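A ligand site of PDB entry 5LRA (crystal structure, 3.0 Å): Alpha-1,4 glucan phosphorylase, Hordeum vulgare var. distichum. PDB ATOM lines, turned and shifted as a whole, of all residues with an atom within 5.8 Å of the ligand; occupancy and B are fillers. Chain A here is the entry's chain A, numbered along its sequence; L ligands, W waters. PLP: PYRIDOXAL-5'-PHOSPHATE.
Water W2 lies within hydrogen-bond range of the side-chain hydroxyl (OH) of Tyr 740, an oxygen (O4P) of the ligand and the backbone carbonyl oxygen (O) of Val 655. Water W1 lies within hydrogen-bond range of NZ of Lys 662 (2.8 Å), NE of Arg 657 (3.1 Å) and O3P of the ligand (3.2 Å).
Leu 95 touches the ligand. C of Gly 139 touches C6 of the ligand, 3.9 Å away. Gly 140 touches the ligand (CA to C5A, 3.6 Å). CG of Arg 143 touches C4A of the ligand (3.9 Å). Trp 578 touches the ligand (CZ2 to O3, 3.6 Å). CE2 of Tyr 740 touches N1 of the ligand (3.9 Å). Asn 741 touches the ligand. Val 742 touches the ligand (N to C2A, 3.3 Å). Ala 745 touches the ligand (CB to O3, 3.98 Å). Gly 767 touches the ligand. Asn 770 touches the ligand. 16 residues have an atom within 4 Å of the ligand: Leu 95, Gly 139, Gly 140, Arg 143, Trp 578, Lys 656, Lys 662, Tyr 740, Asn 741, Val 742, Ala 745, Gly 767, Thr 768, Ser 769, Asn 770 and Lys 772.
The side-chain amino group (NZ) of Lys 772 is bonded to a carbon (C4A) of the ligand (1.3 Å). An oxygen (O2P) of the ligand sits close to the backbone NH (N) of Ser 769 (3.2 Å). The side-chain hydroxyl (OG) of Ser 769 lies within hydrogen-bond range of an oxygen (O2P) of the ligand, 2.5 Å away. The side-chain amino group of Lys 656 lies within salt-bridge range of an oxygen (O2P) of the ligand, 2.9 Å away. The backbone NH (N) of Thr 768 lies within hydrogen-bond range of an oxygen (O1P) of the ligand (3.3 Å). NZ of Lys 662 is in salt-bridge range of O3P of the ligand, 3.3 Å away.
The side-chain amino group (NZ) of Lys 656 lies within hydrogen-bond range of the side-chain hydroxyl (OG) of Ser 769 (3.0 Å). The side-chain amino group of Lys 656 lies within hydrogen-bond range of a ring nitrogen (ND1) of His 757 (3.5 Å). NZ of Lys 662 lies within salt-bridge range of OE1 of Glu 764 (3.4 Å). The guanidinium group of Arg 143 is in hydrogen-bond range of the backbone carbonyl oxygen of Leu 95 (3.0 Å). OD1 of Asn 770 lies within hydrogen-bond range of ND1 of His 757.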
ATOM      1  N   LEU A  95      12.928  25.020 -12.302  1.00  0.00           N
ATOM      2  CA  LEU A  95      13.061  23.619 -11.917  1.00  0.00           C
ATOM      3  C   LEU A  95      14.250  23.013 -12.686  1.00  0.00           C
ATOM      4  O   LEU A  95      14.069  22.289 -13.664  1.00  0.00           O
ATOM      5  CB  LEU A  95      11.779  22.811 -12.209  1.00  0.00           C
ATOM      6  CG  LEU A  95      10.603  22.790 -11.227  1.00  0.00           C
ATOM      7  CD1 LEU A  95       9.532  21.841 -11.750  1.00  0.00           C
ATOM      8  CD2 LEU A  95      11.036  22.366  -9.828  1.00  0.00           C
ATOM      9  N   ASN A 138       8.682  25.157  -8.957  1.00  0.00           N
ATOM     10  CA  ASN A 138       7.416  24.603  -8.499  1.00  0.00           C
ATOM     11  C   ASN A 138       6.706  23.887  -9.640  1.00  0.00           C
ATOM     12  O   ASN A 138       6.563  22.670  -9.613  1.00  0.00           O
ATOM     13  CB  ASN A 138       6.556  25.746  -7.933  1.00  0.00           C
ATOM     14  CG  ASN A 138       5.220  25.281  -7.364  1.00  0.00           C
ATOM     15  OD1 ASN A 138       4.353  26.095  -7.057  1.00  0.00           O
ATOM     16  ND2 ASN A 138       5.056  23.969  -7.194  1.00  0.00           N
ATOM     17  N   GLY A 139       6.290  24.628 -10.657  1.00  0.00           N
ATOM     18  CA  GLY A 139       5.477  24.058 -11.734  1.00  0.00           C
ATOM     19  C   GLY A 139       6.083  24.188 -13.116  1.00  0.00           C
ATOM     20  O   GLY A 139       7.307  24.342 -13.259  1.00  0.00           O
ATOM     21  N   GLY A 140       5.207  24.124 -14.124  1.00  0.00           N
ATOM     22  CA  GLY A 140       5.626  24.234 -15.513  1.00  0.00           C
ATOM     23  C   GLY A 140       6.498  25.456 -15.746  1.00  0.00           C
ATOM     24  O   GLY A 140       7.549  25.366 -16.372  1.00  0.00           O
ATOM     25  N   ARG A 143      10.068  24.650 -14.950  1.00  0.00           N
ATOM     26  CA  ARG A 143      10.636  23.611 -15.802  1.00  0.00           C
ATOM     27  C   ARG A 143      10.724  24.094 -17.250  1.00  0.00           C
ATOM     28  O   ARG A 143      11.612  23.681 -17.983  1.00  0.00           O
ATOM     29  CB  ARG A 143       9.787  22.360 -15.709  1.00  0.00           C
ATOM     30  CG  ARG A 143      10.260  21.171 -16.520  1.00  0.00           C
ATOM     31  CD  ARG A 143      11.653  20.739 -16.120  1.00  0.00           C
ATOM     32  NE  ARG A 143      12.612  20.910 -17.210  1.00  0.00           N
ATOM     33  CZ  ARG A 143      13.929  20.743 -17.102  1.00  0.00           C
ATOM     34  NH1 ARG A 143      14.482  20.423 -15.941  1.00  0.00           N
ATOM     35  NH2 ARG A 143      14.695  20.914 -18.167  1.00  0.00           N
ATOM     36  N   TRP A 578      14.416  14.687 -21.329  1.00  0.00           N
ATOM     37  CA  TRP A 578      13.105  14.031 -21.266  1.00  0.00           C
ATOM     38  C   TRP A 578      12.882  12.836 -22.206  1.00  0.00           C
ATOM     39  O   TRP A 578      11.794  12.258 -22.237  1.00  0.00           O
ATOM     40  CB  TRP A 578      11.976  15.070 -21.396  1.00  0.00           C
ATOM     41  CG  TRP A 578      11.942  16.007 -20.207  1.00  0.00           C
ATOM     42  CD1 TRP A 578      12.136  17.360 -20.217  1.00  0.00           C
ATOM     43  CD2 TRP A 578      11.730  15.651 -18.826  1.00  0.00           C
ATOM     44  NE1 TRP A 578      12.039  17.871 -18.944  1.00  0.00           N
ATOM     45  CE2 TRP A 578      11.797  16.838 -18.068  1.00  0.00           C
ATOM     46  CE3 TRP A 578      11.483  14.444 -18.161  1.00  0.00           C
ATOM     47  CZ2 TRP A 578      11.624  16.848 -16.690  1.00  0.00           C
ATOM     48  CZ3 TRP A 578      11.321  14.463 -16.793  1.00  0.00           C
ATOM     49  CH2 TRP A 578      11.394  15.660 -16.069  1.00  0.00           C
ATOM     50  N   VAL A 655       0.346  13.266 -12.522  1.00  0.00           N
ATOM     51  CA  VAL A 655       1.259  13.982 -11.667  1.00  0.00           C
ATOM     52  C   VAL A 655       1.272  15.450 -12.060  1.00  0.00           C
ATOM     53  O   VAL A 655       1.703  15.809 -13.162  1.00  0.00           O
ATOM     54  CB  VAL A 655       2.673  13.354 -11.669  1.00  0.00           C
ATOM     55  CG1 VAL A 655       2.681  12.079 -10.838  1.00  0.00           C
ATOM     56  CG2 VAL A 655       3.171  13.067 -13.080  1.00  0.00           C
ATOM     57  N   LYS A 656       0.748  16.293 -11.172  1.00  0.00           N
ATOM     58  CA  LYS A 656       0.740  17.738 -11.386  1.00  0.00           C
ATOM     59  C   LYS A 656       0.255  18.486 -10.146  1.00  0.00           C
ATOM     60  O   LYS A 656      -0.456  17.913  -9.316  1.00  0.00           O
ATOM     61  CB  LYS A 656      -0.113  18.119 -12.610  1.00  0.00           C
ATOM     62  CG  LYS A 656      -1.492  17.459 -12.676  1.00  0.00           C
ATOM     63  CD  LYS A 656      -2.091  17.525 -14.075  1.00  0.00           C
ATOM     64  CE  LYS A 656      -1.377  16.635 -15.096  1.00  0.00           C
ATOM     65  NZ  LYS A 656      -0.392  17.363 -15.944  1.00  0.00           N
ATOM     66  N   ARG A 657       0.645  19.756 -10.051  1.00  0.00           N
ATOM     67  CA  ARG A 657       0.212  20.628  -8.953  1.00  0.00           C
ATOM     68  C   ARG A 657      -1.245  20.340  -8.586  1.00  0.00           C
ATOM     69  O   ARG A 657      -2.096  20.232  -9.464  1.00  0.00           O
ATOM     70  CB  ARG A 657       0.418  22.115  -9.316  1.00  0.00           C
ATOM     71  CG  ARG A 657       1.822  22.467  -9.827  1.00  0.00           C
ATOM     72  CD  ARG A 657       2.092  23.977  -9.854  1.00  0.00           C
ATOM     73  NE  ARG A 657       1.243  24.713 -10.807  1.00  0.00           N
ATOM     74  CZ  ARG A 657       0.102  25.351 -10.500  1.00  0.00           C
ATOM     75  NH1 ARG A 657      -0.570  25.989 -11.461  1.00  0.00           N
ATOM     76  NH2 ARG A 657      -0.370  25.383  -9.257  1.00  0.00           N
ATOM     77  N   LYS A 662      -7.243  21.264 -12.039  1.00  0.00           N
ATOM     78  CA  LYS A 662      -6.560  20.178 -12.754  1.00  0.00           C
ATOM     79  C   LYS A 662      -7.334  18.880 -12.538  1.00  0.00           C
ATOM     80  O   LYS A 662      -7.226  17.938 -13.326  1.00  0.00           O
ATOM     81  CB  LYS A 662      -5.104  20.064 -12.311  1.00  0.00           C
ATOM     82  CG  LYS A 662      -4.347  21.383 -12.477  1.00  0.00           C
ATOM     83  CD  LYS A 662      -2.944  21.204 -13.029  1.00  0.00           C
ATOM     84  CE  LYS A 662      -2.375  22.538 -13.482  1.00  0.00           C
ATOM     85  NZ  LYS A 662      -0.902  22.543 -13.701  1.00  0.00           N
ATOM     86  N   TYR A 740       6.755  15.026  -5.363  1.00  0.00           N
ATOM     87  CA  TYR A 740       6.909  14.942  -6.796  1.00  0.00           C
ATOM     88  C   TYR A 740       7.762  16.109  -7.271  1.00  0.00           C
ATOM     89  O   TYR A 740       7.480  17.272  -6.967  1.00  0.00           O
ATOM     90  CB  TYR A 740       5.542  14.926  -7.487  1.00  0.00           C
ATOM     91  CG  TYR A 740       5.614  15.028  -8.979  1.00  0.00           C
ATOM     92  CD1 TYR A 740       6.095  13.978  -9.756  1.00  0.00           C
ATOM     93  CD2 TYR A 740       5.209  16.185  -9.623  1.00  0.00           C
ATOM     94  CE1 TYR A 740       6.161  14.073 -11.131  1.00  0.00           C
ATOM     95  CE2 TYR A 740       5.269  16.303 -11.003  1.00  0.00           C
ATOM     96  CZ  TYR A 740       5.748  15.245 -11.760  1.00  0.00           C
ATOM     97  OH  TYR A 740       5.806  15.380 -13.138  1.00  0.00           O
ATOM     98  N   ASN A 741       8.823  15.790  -7.999  1.00  0.00           N
ATOM     99  CA  ASN A 741       9.773  16.770  -8.502  1.00  0.00           C
ATOM    100  C   ASN A 741      10.435  16.251  -9.774  1.00  0.00           C
ATOM    101  O   ASN A 741      10.154  15.128 -10.201  1.00  0.00           O
ATOM    102  CB  ASN A 741      10.824  17.057  -7.421  1.00  0.00           C
ATOM    103  CG  ASN A 741      11.583  15.814  -7.011  1.00  0.00           C
ATOM    104  OD1 ASN A 741      11.649  14.830  -7.752  1.00  0.00           O
ATOM    105  ND2 ASN A 741      12.173  15.852  -5.832  1.00  0.00           N
ATOM    106  N   VAL A 742      11.327  17.040 -10.349  1.00  0.00           N
ATOM    107  CA  VAL A 742      12.017  16.650 -11.576  1.00  0.00           C
ATOM    108  C   VAL A 742      12.523  15.202 -11.481  1.00  0.00           C
ATOM    109  O   VAL A 742      12.202  14.376 -12.334  1.00  0.00           O
ATOM    110  CB  VAL A 742      13.187  17.598 -11.912  1.00  0.00           C
ATOM    111  CG1 VAL A 742      13.790  17.235 -13.261  1.00  0.00           C
ATOM    112  CG2 VAL A 742      12.727  19.045 -11.916  1.00  0.00           C
ATOM    113  N   ALA A 745       9.743  12.637 -11.679  1.00  0.00           N
ATOM    114  CA  ALA A 745       9.179  12.609 -13.021  1.00  0.00           C
ATOM    115  C   ALA A 745      10.087  11.828 -13.989  1.00  0.00           C
ATOM    116  O   ALA A 745       9.604  11.156 -14.887  1.00  0.00           O
ATOM    117  CB  ALA A 745       8.949  14.017 -13.528  1.00  0.00           C
ATOM    118  N   ILE A 749       7.771   9.043 -15.666  1.00  0.00           N
ATOM    119  CA  ILE A 749       7.321   9.309 -17.043  1.00  0.00           C
ATOM    120  C   ILE A 749       7.648   8.197 -18.049  1.00  0.00           C
ATOM    121  O   ILE A 749       6.739   7.646 -18.671  1.00  0.00           O
ATOM    122  CB  ILE A 749       7.829  10.685 -17.548  1.00  0.00           C
ATOM    123  CG1 ILE A 749       6.972  11.796 -16.955  1.00  0.00           C
ATOM    124  CG2 ILE A 749       7.802  10.768 -19.076  1.00  0.00           C
ATOM    125  CD1 ILE A 749       7.559  13.194 -17.090  1.00  0.00           C
ATOM    126  N   HIS A 757      -4.488  14.303 -18.319  1.00  0.00           N
ATOM    127  CA  HIS A 757      -4.408  15.741 -18.422  1.00  0.00           C
ATOM    128  C   HIS A 757      -5.842  16.182 -18.639  1.00  0.00           C
ATOM    129  O   HIS A 757      -6.261  16.486 -19.765  1.00  0.00           O
ATOM    130  CB  HIS A 757      -3.497  16.130 -19.584  1.00  0.00           C
ATOM    131  CG  HIS A 757      -2.206  15.386 -19.586  1.00  0.00           C
ATOM    132  ND1 HIS A 757      -1.060  15.895 -19.026  1.00  0.00           N
ATOM    133  CD2 HIS A 757      -1.893  14.135 -20.015  1.00  0.00           C
ATOM    134  CE1 HIS A 757      -0.084  15.008 -19.135  1.00  0.00           C
ATOM    135  NE2 HIS A 757      -0.572  13.932 -19.723  1.00  0.00           N
ATOM    136  N   GLU A 764      -6.268  25.286 -18.436  1.00  0.00           N
ATOM    137  CA  GLU A 764      -4.862  25.030 -18.690  1.00  0.00           C
ATOM    138  C   GLU A 764      -4.434  25.835 -19.903  1.00  0.00           C
ATOM    139  O   GLU A 764      -5.101  25.794 -20.950  1.00  0.00           O
ATOM    140  CB  GLU A 764      -4.629  23.544 -18.965  1.00  0.00           C
ATOM    141  CG  GLU A 764      -3.211  23.102 -18.716  1.00  0.00           C
ATOM    142  CD  GLU A 764      -2.961  22.858 -17.252  1.00  0.00           C
ATOM    143  OE1 GLU A 764      -2.191  23.627 -16.641  1.00  0.00           O
ATOM    144  OE2 GLU A 764      -3.565  21.903 -16.711  1.00  0.00           O
ATOM    145  N   SER A 766      -1.128  25.698 -21.398  1.00  0.00           N
ATOM    146  CA  SER A 766      -0.436  24.734 -22.257  1.00  0.00           C
ATOM    147  C   SER A 766      -0.268  23.403 -21.570  1.00  0.00           C
ATOM    148  O   SER A 766      -0.910  22.429 -21.936  1.00  0.00           O
ATOM    149  CB  SER A 766       0.940  25.239 -22.685  1.00  0.00           C
ATOM    150  OG  SER A 766       1.697  24.208 -23.298  1.00  0.00           O
ATOM    151  N   GLY A 767       0.630  23.366 -20.586  1.00  0.00           N
ATOM    152  CA  GLY A 767       1.036  22.121 -19.948  1.00  0.00           C
ATOM    153  C   GLY A 767       2.178  21.455 -20.712  1.00  0.00           C
ATOM    154  O   GLY A 767       2.147  21.328 -21.928  1.00  0.00           O
ATOM    155  N   THR A 768       3.202  21.023 -19.968  1.00  0.00           N
ATOM    156  CA  THR A 768       4.385  20.447 -20.575  1.00  0.00           C
ATOM    157  C   THR A 768       4.580  18.984 -20.278  1.00  0.00           C
ATOM    158  O   THR A 768       5.289  18.316 -21.015  1.00  0.00           O
ATOM    159  CB  THR A 768       5.641  21.191 -20.099  1.00  0.00           C
ATOM    160  OG1 THR A 768       5.584  21.353 -18.688  1.00  0.00           O
ATOM    161  CG2 THR A 768       5.747  22.556 -20.771  1.00  0.00           C
ATOM    162  N   SER A 769       3.992  18.465 -19.201  1.00  0.00           N
ATOM    163  CA  SER A 769       4.136  17.029 -18.917  1.00  0.00           C
ATOM    164  C   SER A 769       3.456  16.257 -20.033  1.00  0.00           C
ATOM    165  O   SER A 769       3.934  15.203 -20.435  1.00  0.00           O
ATOM    166  CB  SER A 769       3.571  16.647 -17.531  1.00  0.00           C
ATOM    167  OG  SER A 769       2.158  16.730 -17.488  1.00  0.00           O
ATOM    168  N   ASN A 770       2.364  16.817 -20.538  1.00  0.00           N
ATOM    169  CA  ASN A 770       1.709  16.298 -21.734  1.00  0.00           C
ATOM    170  C   ASN A 770       2.726  15.818 -22.744  1.00  0.00           C
ATOM    171  O   ASN A 770       2.668  14.688 -23.241  1.00  0.00           O
ATOM    172  CB  ASN A 770       0.903  17.408 -22.415  1.00  0.00           C
ATOM    173  CG  ASN A 770       0.074  18.202 -21.450  1.00  0.00           C
ATOM    174  OD1 ASN A 770       0.453  18.400 -20.293  1.00  0.00           O
ATOM    175  ND2 ASN A 770      -1.074  18.666 -21.921  1.00  0.00           N
ATOM    176  N   LYS A 772       6.078  15.531 -22.437  1.00  0.00           N
ATOM    177  CA  LYS A 772       7.058  14.579 -21.912  1.00  0.00           C
ATOM    178  C   LYS A 772       6.532  13.163 -22.070  1.00  0.00           C
ATOM    179  O   LYS A 772       7.254  12.279 -22.520  1.00  0.00           O
ATOM    180  CB  LYS A 772       7.354  14.847 -20.425  1.00  0.00           C
ATOM    181  CG  LYS A 772       7.969  16.200 -20.135  1.00  0.00           C
ATOM    182  CD  LYS A 772       8.054  16.496 -18.646  1.00  0.00           C
ATOM    183  CE  LYS A 772       8.382  17.964 -18.404  1.00  0.00           C
ATOM    184  NZ  LYS A 772       8.121  18.381 -17.006  1.00  0.00           N
HETATM  185  N1  PLP L   1       6.654  19.718 -12.340  1.00  0.00           N
HETATM  186  C2  PLP L   1       7.673  18.934 -12.741  1.00  0.00           C
HETATM  187  C2A PLP L   1       8.647  18.324 -11.779  1.00  0.00           C
HETATM  188  C3  PLP L   1       7.854  18.642 -14.170  1.00  0.00           C
HETATM  189  O3  PLP L   1       8.889  17.854 -14.566  1.00  0.00           O
HETATM  190  C4  PLP L   1       6.902  19.225 -15.121  1.00  0.00           C
HETATM  191  C4A PLP L   1       7.071  18.949 -16.559  1.00  0.00           C
HETATM  192  C5  PLP L   1       5.818  20.081 -14.556  1.00  0.00           C
HETATM  193  C6  PLP L   1       5.768  20.265 -13.169  1.00  0.00           C
HETATM  194  C5A PLP L   1       4.747  20.723 -15.418  1.00  0.00           C
HETATM  195  O4P PLP L   1       3.630  19.817 -15.632  1.00  0.00           O
HETATM  196  P   PLP L   1       2.134  20.258 -16.111  1.00  0.00           P
HETATM  197  O1P PLP L   1       2.296  21.580 -16.839  1.00  0.00           O
HETATM  198  O2P PLP L   1       1.725  19.120 -17.006  1.00  0.00           O
HETATM  199  O3P PLP L   1       1.309  20.326 -14.838  1.00  0.00           O
HETATM  200  O   HOH W   1       1.828  23.123 -13.411  1.00  0.00           O
HETATM  201  O   HOH W   2       4.030  17.386 -14.070  1.00  0.00           O
